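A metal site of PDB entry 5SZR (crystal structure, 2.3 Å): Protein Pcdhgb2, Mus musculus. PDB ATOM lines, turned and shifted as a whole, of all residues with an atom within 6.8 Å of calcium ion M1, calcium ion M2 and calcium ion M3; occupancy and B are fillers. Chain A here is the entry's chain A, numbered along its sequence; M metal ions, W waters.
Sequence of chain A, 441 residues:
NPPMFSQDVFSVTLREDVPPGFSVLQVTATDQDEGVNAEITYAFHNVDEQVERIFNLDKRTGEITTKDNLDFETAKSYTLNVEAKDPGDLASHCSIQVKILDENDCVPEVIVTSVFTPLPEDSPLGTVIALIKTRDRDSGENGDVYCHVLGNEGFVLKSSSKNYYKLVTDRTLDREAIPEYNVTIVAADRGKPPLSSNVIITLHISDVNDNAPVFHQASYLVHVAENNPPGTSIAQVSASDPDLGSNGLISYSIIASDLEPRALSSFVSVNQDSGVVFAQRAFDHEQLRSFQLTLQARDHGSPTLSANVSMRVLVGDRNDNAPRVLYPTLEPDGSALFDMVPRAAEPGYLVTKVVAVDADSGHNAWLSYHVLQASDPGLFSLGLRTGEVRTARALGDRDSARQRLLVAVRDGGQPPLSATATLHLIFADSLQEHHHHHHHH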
ATOM      1  N   GLU A  16       0.740   2.195  24.514  1.00  0.00           N
ATOM      2  CA  GLU A  16       0.494   3.633  24.539  1.00  0.00           C
ATOM      3  C   GLU A  16      -0.948   4.009  24.197  1.00  0.00           C
ATOM      4  O   GLU A  16      -1.333   5.160  24.413  1.00  0.00           O
ATOM      5  CB  GLU A  16       1.452   4.363  23.600  1.00  0.00           C
ATOM      6  CG  GLU A  16       1.359   3.949  22.138  1.00  0.00           C
ATOM      7  CD  GLU A  16       2.070   4.927  21.217  1.00  0.00           C
ATOM      8  OE1 GLU A  16       2.152   6.130  21.556  1.00  0.00           O
ATOM      9  OE2 GLU A  16       2.561   4.501  20.159  1.00  0.00           O
ATOM     10  N   LEU A  70      -1.762   8.134  27.079  1.00  0.00           N
ATOM     11  CA  LEU A  70      -0.334   7.911  26.970  1.00  0.00           C
ATOM     12  C   LEU A  70       0.166   8.316  25.587  1.00  0.00           C
ATOM     13  O   LEU A  70      -0.617   8.648  24.687  1.00  0.00           O
ATOM     14  CB  LEU A  70       0.005   6.452  27.271  1.00  0.00           C
ATOM     15  CG  LEU A  70      -0.475   5.931  28.639  1.00  0.00           C
ATOM     16  CD1 LEU A  70      -0.044   4.490  28.893  1.00  0.00           C
ATOM     17  CD2 LEU A  70       0.008   6.839  29.756  1.00  0.00           C
ATOM     18  N   ASP A  71       1.487   8.318  25.427  1.00  0.00           N
ATOM     19  CA  ASP A  71       2.116   8.636  24.155  1.00  0.00           C
ATOM     20  C   ASP A  71       3.591   8.226  24.198  1.00  0.00           C
ATOM     21  O   ASP A  71       4.404   8.891  24.847  1.00  0.00           O
ATOM     22  CB  ASP A  71       1.991  10.133  23.827  1.00  0.00           C
ATOM     23  CG  ASP A  71       2.653  10.516  22.520  1.00  0.00           C
ATOM     24  OD1 ASP A  71       2.891   9.630  21.677  1.00  0.00           O
ATOM     25  OD2 ASP A  71       2.921  11.720  22.329  1.00  0.00           O
ATOM     26  N   PHE A  72       3.922   7.114  23.530  1.00  0.00           N
ATOM     27  CA  PHE A  72       5.293   6.606  23.534  1.00  0.00           C
ATOM     28  C   PHE A  72       6.265   7.630  22.972  1.00  0.00           C
ATOM     29  O   PHE A  72       7.420   7.681  23.391  1.00  0.00           O
ATOM     30  CB  PHE A  72       5.348   5.305  22.727  1.00  0.00           C
ATOM     31  CG  PHE A  72       6.723   4.716  22.610  1.00  0.00           C
ATOM     32  CD1 PHE A  72       7.204   3.853  23.577  1.00  0.00           C
ATOM     33  CD2 PHE A  72       7.541   5.020  21.520  1.00  0.00           C
ATOM     34  CE1 PHE A  72       8.464   3.298  23.468  1.00  0.00           C
ATOM     35  CE2 PHE A  72       8.801   4.465  21.411  1.00  0.00           C
ATOM     36  CZ  PHE A  72       9.272   3.600  22.388  1.00  0.00           C
ATOM     37  N   GLU A  73       5.817   8.453  22.017  1.00  0.00           N
ATOM     38  CA  GLU A  73       6.702   9.439  21.425  1.00  0.00           C
ATOM     39  C   GLU A  73       7.052  10.555  22.403  1.00  0.00           C
ATOM     40  O   GLU A  73       8.062  11.240  22.205  1.00  0.00           O
ATOM     41  CB  GLU A  73       6.055  10.020  20.156  1.00  0.00           C
ATOM     42  CG  GLU A  73       6.140   9.115  18.923  1.00  0.00           C
ATOM     43  CD  GLU A  73       5.457   7.757  19.107  1.00  0.00           C
ATOM     44  OE1 GLU A  73       4.308   7.723  19.586  1.00  0.00           O
ATOM     45  OE2 GLU A  73       6.085   6.734  18.763  1.00  0.00           O
ATOM     46  N   THR A  74       6.250  10.746  23.455  1.00  0.00           N
ATOM     47  CA  THR A  74       6.505  11.753  24.479  1.00  0.00           C
ATOM     48  C   THR A  74       7.224  11.195  25.702  1.00  0.00           C
ATOM     49  O   THR A  74       8.128  11.832  26.235  1.00  0.00           O
ATOM     50  CB  THR A  74       5.181  12.404  24.919  1.00  0.00           C
ATOM     51  OG1 THR A  74       4.499  12.939  23.785  1.00  0.00           O
ATOM     52  CG2 THR A  74       5.438  13.516  25.919  1.00  0.00           C
ATOM     53  N   LEU A 101       4.863   0.748  25.624  1.00  0.00           N
ATOM     54  CA  LEU A 101       5.098   0.035  24.375  1.00  0.00           C
ATOM     55  C   LEU A 101       4.712   0.902  23.184  1.00  0.00           C
ATOM     56  O   LEU A 101       3.679   1.578  23.207  1.00  0.00           O
ATOM     57  CB  LEU A 101       4.321  -1.286  24.343  1.00  0.00           C
ATOM     58  CG  LEU A 101       4.810  -2.308  25.363  1.00  0.00           C
ATOM     59  CD1 LEU A 101       3.955  -3.563  25.321  1.00  0.00           C
ATOM     60  CD2 LEU A 101       6.275  -2.634  25.112  1.00  0.00           C
ATOM     61  N   ASP A 102       5.551   0.886  22.154  1.00  0.00           N
ATOM     62  CA  ASP A 102       5.318   1.695  20.976  1.00  0.00           C
ATOM     63  C   ASP A 102       4.257   1.050  20.080  1.00  0.00           C
ATOM     64  O   ASP A 102       4.356  -0.131  19.740  1.00  0.00           O
ATOM     65  CB  ASP A 102       6.616   1.874  20.187  1.00  0.00           C
ATOM     66  CG  ASP A 102       6.395   2.434  18.802  1.00  0.00           C
ATOM     67  OD1 ASP A 102       5.609   3.394  18.664  1.00  0.00           O
ATOM     68  OD2 ASP A 102       7.000   1.911  17.839  1.00  0.00           O
ATOM     69  N   GLU A 103       3.248   1.834  19.719  1.00  0.00           N
ATOM     70  CA  GLU A 103       2.260   1.451  18.722  1.00  0.00           C
ATOM     71  C   GLU A 103       2.444   2.301  17.471  1.00  0.00           C
ATOM     72  O   GLU A 103       3.002   3.406  17.517  1.00  0.00           O
ATOM     73  CB  GLU A 103       0.830   1.631  19.258  1.00  0.00           C
ATOM     74  CG  GLU A 103       0.520   0.845  20.533  1.00  0.00           C
ATOM     75  CD  GLU A 103       0.460  -0.655  20.300  1.00  0.00           C
ATOM     76  OE1 GLU A 103       0.985  -1.405  21.156  1.00  0.00           O
ATOM     77  OE2 GLU A 103      -0.094  -1.069  19.270  1.00  0.00           O
ATOM     78  N   ASN A 104       1.962   1.766  16.356  1.00  0.00           N
ATOM     79  CA  ASN A 104       2.046   2.448  15.064  1.00  0.00           C
ATOM     80  C   ASN A 104       0.908   3.465  14.993  1.00  0.00           C
ATOM     81  O   ASN A 104      -0.183   3.175  14.496  1.00  0.00           O
ATOM     82  CB  ASN A 104       1.981   1.439  13.924  1.00  0.00           C
ATOM     83  CG  ASN A 104       2.280   2.052  12.583  1.00  0.00           C
ATOM     84  OD1 ASN A 104       2.733   3.196  12.483  1.00  0.00           O
ATOM     85  ND2 ASN A 104       2.041   1.295  11.520  1.00  0.00           N
ATOM     86  N   ASP A 105       1.151   4.670  15.500  1.00  0.00           N
ATOM     87  CA  ASP A 105       0.154   5.725  15.471  1.00  0.00           C
ATOM     88  C   ASP A 105       0.664   7.018  14.838  1.00  0.00           C
ATOM     89  O   ASP A 105      -0.007   8.046  14.949  1.00  0.00           O
ATOM     90  CB  ASP A 105      -0.385   6.008  16.883  1.00  0.00           C
ATOM     91  CG  ASP A 105       0.694   6.432  17.856  1.00  0.00           C
ATOM     92  OD1 ASP A 105       1.882   6.222  17.577  1.00  0.00           O
ATOM     93  OD2 ASP A 105       0.337   6.971  18.926  1.00  0.00           O
ATOM     94  N   CYS A 106       1.823   6.988  14.180  1.00  0.00           N
ATOM     95  CA  CYS A 106       2.376   8.155  13.493  1.00  0.00           C
ATOM     96  C   CYS A 106       2.515   7.848  12.017  1.00  0.00           C
ATOM     97  O   CYS A 106       3.183   6.879  11.633  1.00  0.00           O
ATOM     98  CB  CYS A 106       3.728   8.554  14.090  1.00  0.00           C
ATOM     99  SG  CYS A 106       3.630   9.294  15.745  1.00  0.00           S
ATOM    100  N   VAL A 107       1.877   8.669  11.187  1.00  0.00           N
ATOM    101  CA  VAL A 107       1.867   8.461   9.729  1.00  0.00           C
ATOM    102  C   VAL A 107       3.244   8.824   9.170  1.00  0.00           C
ATOM    103  O   VAL A 107       3.893   9.737   9.691  1.00  0.00           O
ATOM    104  CB  VAL A 107       0.760   9.304   9.085  1.00  0.00           C
ATOM    105  CG1 VAL A 107       0.778   9.199   7.567  1.00  0.00           C
ATOM    106  CG2 VAL A 107      -0.602   8.882   9.636  1.00  0.00           C
ATOM    107  N   PRO A 108       3.730   8.114   8.145  1.00  0.00           N
ATOM    108  CA  PRO A 108       4.940   8.588   7.454  1.00  0.00           C
ATOM    109  C   PRO A 108       4.659   9.877   6.693  1.00  0.00           C
ATOM    110  O   PRO A 108       3.571  10.076   6.155  1.00  0.00           O
ATOM    111  CB  PRO A 108       5.272   7.447   6.478  1.00  0.00           C
ATOM    112  CG  PRO A 108       4.478   6.266   6.958  1.00  0.00           C
ATOM    113  CD  PRO A 108       3.267   6.812   7.647  1.00  0.00           C
ATOM    114  N   ASP A 136       9.351   9.438  10.084  1.00  0.00           N
ATOM    115  CA  ASP A 136       8.308   8.677  10.772  1.00  0.00           C
ATOM    116  C   ASP A 136       8.612   8.715  12.262  1.00  0.00           C
ATOM    117  O   ASP A 136       9.660   8.212  12.689  1.00  0.00           O
ATOM    118  CB  ASP A 136       8.245   7.242  10.257  1.00  0.00           C
ATOM    119  CG  ASP A 136       6.968   6.524  10.688  1.00  0.00           C
ATOM    120  OD1 ASP A 136       6.671   6.477  11.905  1.00  0.00           O
ATOM    121  OD2 ASP A 136       6.246   6.024   9.796  1.00  0.00           O
ATOM    122  N   ARG A 137       7.703   9.291  13.042  1.00  0.00           N
ATOM    123  CA  ARG A 137       7.968   9.545  14.454  1.00  0.00           C
ATOM    124  C   ARG A 137       7.965   8.282  15.299  1.00  0.00           C
ATOM    125  O   ARG A 137       8.412   8.332  16.445  1.00  0.00           O
ATOM    126  CB  ARG A 137       6.931  10.535  14.988  1.00  0.00           C
ATOM    127  CG  ARG A 137       6.907  11.879  14.253  1.00  0.00           C
ATOM    128  CD  ARG A 137       6.036  12.874  14.990  1.00  0.00           C
ATOM    129  NE  ARG A 137       6.357  12.893  16.414  1.00  0.00           N
ATOM    130  CZ  ARG A 137       5.594  13.419  17.358  1.00  0.00           C
ATOM    131  NH1 ARG A 137       5.973  13.381  18.629  1.00  0.00           N
ATOM    132  NH2 ARG A 137       4.435  13.997  17.039  1.00  0.00           N
ATOM    133  N   ASP A 138       7.489   7.154  14.767  1.00  0.00           N
ATOM    134  CA  ASP A 138       7.480   5.896  15.490  1.00  0.00           C
ATOM    135  C   ASP A 138       8.866   5.269  15.512  1.00  0.00           C
ATOM    136  O   ASP A 138       9.792   5.700  14.812  1.00  0.00           O
ATOM    137  CB  ASP A 138       6.470   4.926  14.877  1.00  0.00           C
ATOM    138  CG  ASP A 138       5.036   5.373  15.056  1.00  0.00           C
ATOM    139  OD1 ASP A 138       4.754   6.027  16.083  1.00  0.00           O
ATOM    140  OD2 ASP A 138       4.192   5.079  14.181  1.00  0.00           O
ATOM    141  N   SER A 139       9.007   4.218  16.329  1.00  0.00           N
ATOM    142  CA  SER A 139      10.243   3.468  16.480  1.00  0.00           C
ATOM    143  C   SER A 139      10.144   2.128  15.756  1.00  0.00           C
ATOM    144  O   SER A 139       9.058   1.645  15.428  1.00  0.00           O
ATOM    145  CB  SER A 139      10.568   3.223  17.960  1.00  0.00           C
ATOM    146  OG  SER A 139      10.768   4.441  18.654  1.00  0.00           O
ATOM    147  N   GLU A 141       9.963  -1.050  13.487  1.00  0.00           N
ATOM    148  CA  GLU A 141       9.289  -1.315  12.220  1.00  0.00           C
ATOM    149  C   GLU A 141       8.197  -0.289  11.940  1.00  0.00           C
ATOM    150  O   GLU A 141       7.944   0.059  10.784  1.00  0.00           O
ATOM    151  CB  GLU A 141       8.711  -2.733  12.226  1.00  0.00           C
ATOM    152  CG  GLU A 141       9.766  -3.821  12.215  1.00  0.00           C
ATOM    153  CD  GLU A 141       9.179  -5.218  12.119  1.00  0.00           C
ATOM    154  OE1 GLU A 141       7.935  -5.329  11.986  1.00  0.00           O
ATOM    155  OE2 GLU A 141       9.951  -6.193  12.182  1.00  0.00           O
ATOM    156  N   ASN A 142       7.533   0.195  12.996  1.00  0.00           N
ATOM    157  CA  ASN A 142       6.501   1.202  12.807  1.00  0.00           C
ATOM    158  C   ASN A 142       7.055   2.488  12.205  1.00  0.00           C
ATOM    159  O   ASN A 142       6.320   3.238  11.553  1.00  0.00           O
ATOM    160  CB  ASN A 142       5.804   1.483  14.142  1.00  0.00           C
ATOM    161  CG  ASN A 142       5.176   0.233  14.741  1.00  0.00           C
ATOM    162  OD1 ASN A 142       5.224  -0.848  14.149  1.00  0.00           O
ATOM    163  ND2 ASN A 142       4.590   0.379  15.926  1.00  0.00           N
ATOM    164  N   GLY A 143       8.347   2.753  12.395  1.00  0.00           N
ATOM    165  CA  GLY A 143       9.010   3.897  11.796  1.00  0.00           C
ATOM    166  C   GLY A 143       9.824   3.610  10.559  1.00  0.00           C
ATOM    167  O   GLY A 143      10.448   4.528  10.013  1.00  0.00           O
ATOM    168  N   ASP A 144       9.848   2.369  10.087  1.00  0.00           N
ATOM    169  CA  ASP A 144      10.595   1.998   8.897  1.00  0.00           C
ATOM    170  C   ASP A 144       9.726   2.253   7.676  1.00  0.00           C
ATOM    171  O   ASP A 144       8.734   1.543   7.456  1.00  0.00           O
ATOM    172  CB  ASP A 144      11.025   0.529   8.978  1.00  0.00           C
ATOM    173  CG  ASP A 144      12.308   0.265   8.219  1.00  0.00           C
ATOM    174  OD1 ASP A 144      13.257   1.063   8.340  1.00  0.00           O
ATOM    175  OD2 ASP A 144      12.384  -0.764   7.507  1.00  0.00           O
ATOM    176  N   VAL A 145      10.103   3.246   6.868  1.00  0.00           N
ATOM    177  CA  VAL A 145       9.308   3.699   5.738  1.00  0.00           C
ATOM    178  C   VAL A 145      10.023   3.349   4.435  1.00  0.00           C
ATOM    179  O   VAL A 145      11.260   3.382   4.359  1.00  0.00           O
ATOM    180  CB  VAL A 145       9.027   5.215   5.814  1.00  0.00           C
ATOM    181  CG1 VAL A 145       8.093   5.653   4.688  1.00  0.00           C
ATOM    182  CG2 VAL A 145       8.456   5.579   7.156  1.00  0.00           C
ATOM    183  N   ASP A 189       4.739   2.676   6.126  1.00  0.00           N
ATOM    184  CA  ASP A 189       5.557   2.073   7.167  1.00  0.00           C
ATOM    185  C   ASP A 189       5.308   0.563   7.235  1.00  0.00           C
ATOM    186  O   ASP A 189       4.337   0.040   6.683  1.00  0.00           O
ATOM    187  CB  ASP A 189       5.291   2.720   8.540  1.00  0.00           C
ATOM    188  CG  ASP A 189       3.836   2.602   8.990  1.00  0.00           C
ATOM    189  OD1 ASP A 189       3.186   1.561   8.764  1.00  0.00           O
ATOM    190  OD2 ASP A 189       3.337   3.572   9.608  1.00  0.00           O
ATOM    191  N   ARG A 190       6.199  -0.129   7.926  1.00  0.00           N
ATOM    192  CA  ARG A 190       6.106  -1.585   8.041  1.00  0.00           C
ATOM    193  C   ARG A 190       5.670  -1.997   9.443  1.00  0.00           C
ATOM    194  O   ARG A 190       6.256  -2.899  10.051  1.00  0.00           O
ATOM    195  CB  ARG A 190       7.442  -2.225   7.662  1.00  0.00           C
ATOM    196  CG  ARG A 190       7.829  -1.981   6.209  1.00  0.00           C
ATOM    197  CD  ARG A 190       9.181  -2.574   5.865  1.00  0.00           C
ATOM    198  NE  ARG A 190       9.496  -2.431   4.450  1.00  0.00           N
ATOM    199  CZ  ARG A 190       9.543  -3.440   3.580  1.00  0.00           C
ATOM    200  NH1 ARG A 190       9.296  -4.680   3.988  1.00  0.00           N
ATOM    201  NH2 ARG A 190       9.837  -3.212   2.310  1.00  0.00           N
ATOM    202  N   GLY A 191       4.627  -1.348   9.958  1.00  0.00           N
ATOM    203  CA  GLY A 191       4.010  -1.729  11.209  1.00  0.00           C
ATOM    204  C   GLY A 191       2.743  -2.530  10.978  1.00  0.00           C
ATOM    205  O   GLY A 191       2.331  -2.829   9.860  1.00  0.00           O
ATOM    206  N   LEU A 195       0.641   2.146   8.058  1.00  0.00           N
ATOM    207  CA  LEU A 195       0.134   3.463   7.708  1.00  0.00           C
ATOM    208  C   LEU A 195       0.893   4.002   6.515  1.00  0.00           C
ATOM    209  O   LEU A 195       2.076   3.720   6.334  1.00  0.00           O
ATOM    210  CB  LEU A 195       0.256   4.430   8.892  1.00  0.00           C
ATOM    211  CG  LEU A 195      -0.520   4.066  10.165  1.00  0.00           C
ATOM    212  CD1 LEU A 195      -0.172   5.009  11.300  1.00  0.00           C
ATOM    213  CD2 LEU A 195      -2.012   4.087   9.888  1.00  0.00           C
HETATM  214 CA    CA M   1       4.479   4.798  11.647  1.00  0.00          CA
HETATM  215 CA    CA M   2       4.017   5.479  18.397  1.00  0.00          CA
HETATM  216 CA    CA M   3       2.036   8.167  20.031  1.00  0.00          CA
HETATM  217  O   HOH W   1      -0.012   8.792  20.916  1.00  0.00           O
HETATM  218  O   HOH W   2       1.902  10.429  18.488  1.00  0.00           O
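The side-chain carboxylate (OD2) of Asp 102 sits at hydrogen-bond distance from the backbone NH (N) of Ser 139 (3.4 Å).
The backbone NH of Phe 72 lies close to the side-chain carboxylate of Glu 16, at 2.8 Å.
The backbone NH (N) of Glu 16 is in hydrogen-bond range of the backbone carbonyl oxygen (O) of Leu 101 (3.3 Å).
The side-chain amide nitrogen (ND2) of Asn 142 is in hydrogen-bond range of the side-chain carboxylate (OD2) of Asp 102 (3.4 Å).
OD1 of Asp 189 sits at hydrogen-bond distance from N of Leu 195, 2.7 Å away.
OD2 of Asp 71 is in hydrogen-bond range of OG1 of Thr 74, at 2.5 Å.
The side-chain carboxylate (OD1) of Asp 189 sits close to the backbone NH (N) of Gly 191 (3.5 Å).
Six residues have an atom within 4 Å of calcium ion M1: Asn 104, Cys 106, Asp 136, Asp 138, Asn 142 and Asp 189.
The nearest printed residue that does not touch calcium ion M1 is Gly 143 (4.4 Å).
Six residues have an atom within 4 Å of calcium ion M2: Glu 16, Glu 73, Asp 102, Glu 103, Asp 105 and Asp 138.
Along chain A the residues within 4 Å of calcium ion M3 span positions 16 to 105.
O of Asn 142 is bound to calcium ion M1 (2.4 Å).
O of Cys 106 binds calcium ion M1, 2.5 Å away.
OD1 of Asn 104 binds calcium ion M1, at 2.5 Å.
Calcium ion M1 is bound by OD2 of Asp 138 (2.6 Å).
OD2 of Asp 189 binds calcium ion M1 (2.6 Å).
Calcium ion M1 is bound by the side-chain carboxylate (OD1) of Asp 136.
OD2 of Asp 136 binds calcium ion M1, 2.8 Å away.
Calcium ion M1 has seven donor atoms within binding distance.
The side-chain carboxylate (OD1) of Asp 105 binds calcium ion M2, 2.4 Å away.
OE2 of Glu 73 binds calcium ion M2 (2.4 Å).
Calcium ion M2 is bound by O of Glu 103 (2.5 Å).
OE2 of Glu 16 is bound to calcium ion M2 (2.5 Å).
Calcium ion M2 is bound by OD1 of Asp 138, 2.5 Å away.
Calcium ion M2 is bound by the side-chain carboxylate (OE1) of Glu 73, 2.6 Å away.
OD1 of Asp 102 binds calcium ion M2 (2.6 Å).
Calcium ion M3 is bound by water W1 (2.3 Å), the side-chain carboxylate (OD2) of Asp 105 (2.4 Å), the side-chain carboxylate (OE1) of Glu 73 (2.4 Å), the side-chain carboxylate (OD1) of Asp 71 (2.4 Å), the side-chain carboxylate (OE1) of Glu 16 (2.5 Å) and water W2 (2.7 Å).
Calcium ion M3 has six donor atoms within binding distance.
Slightly farther from calcium ion M3 lies the side-chain carboxylate (OD1) of Asp 105 (3.1 Å).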
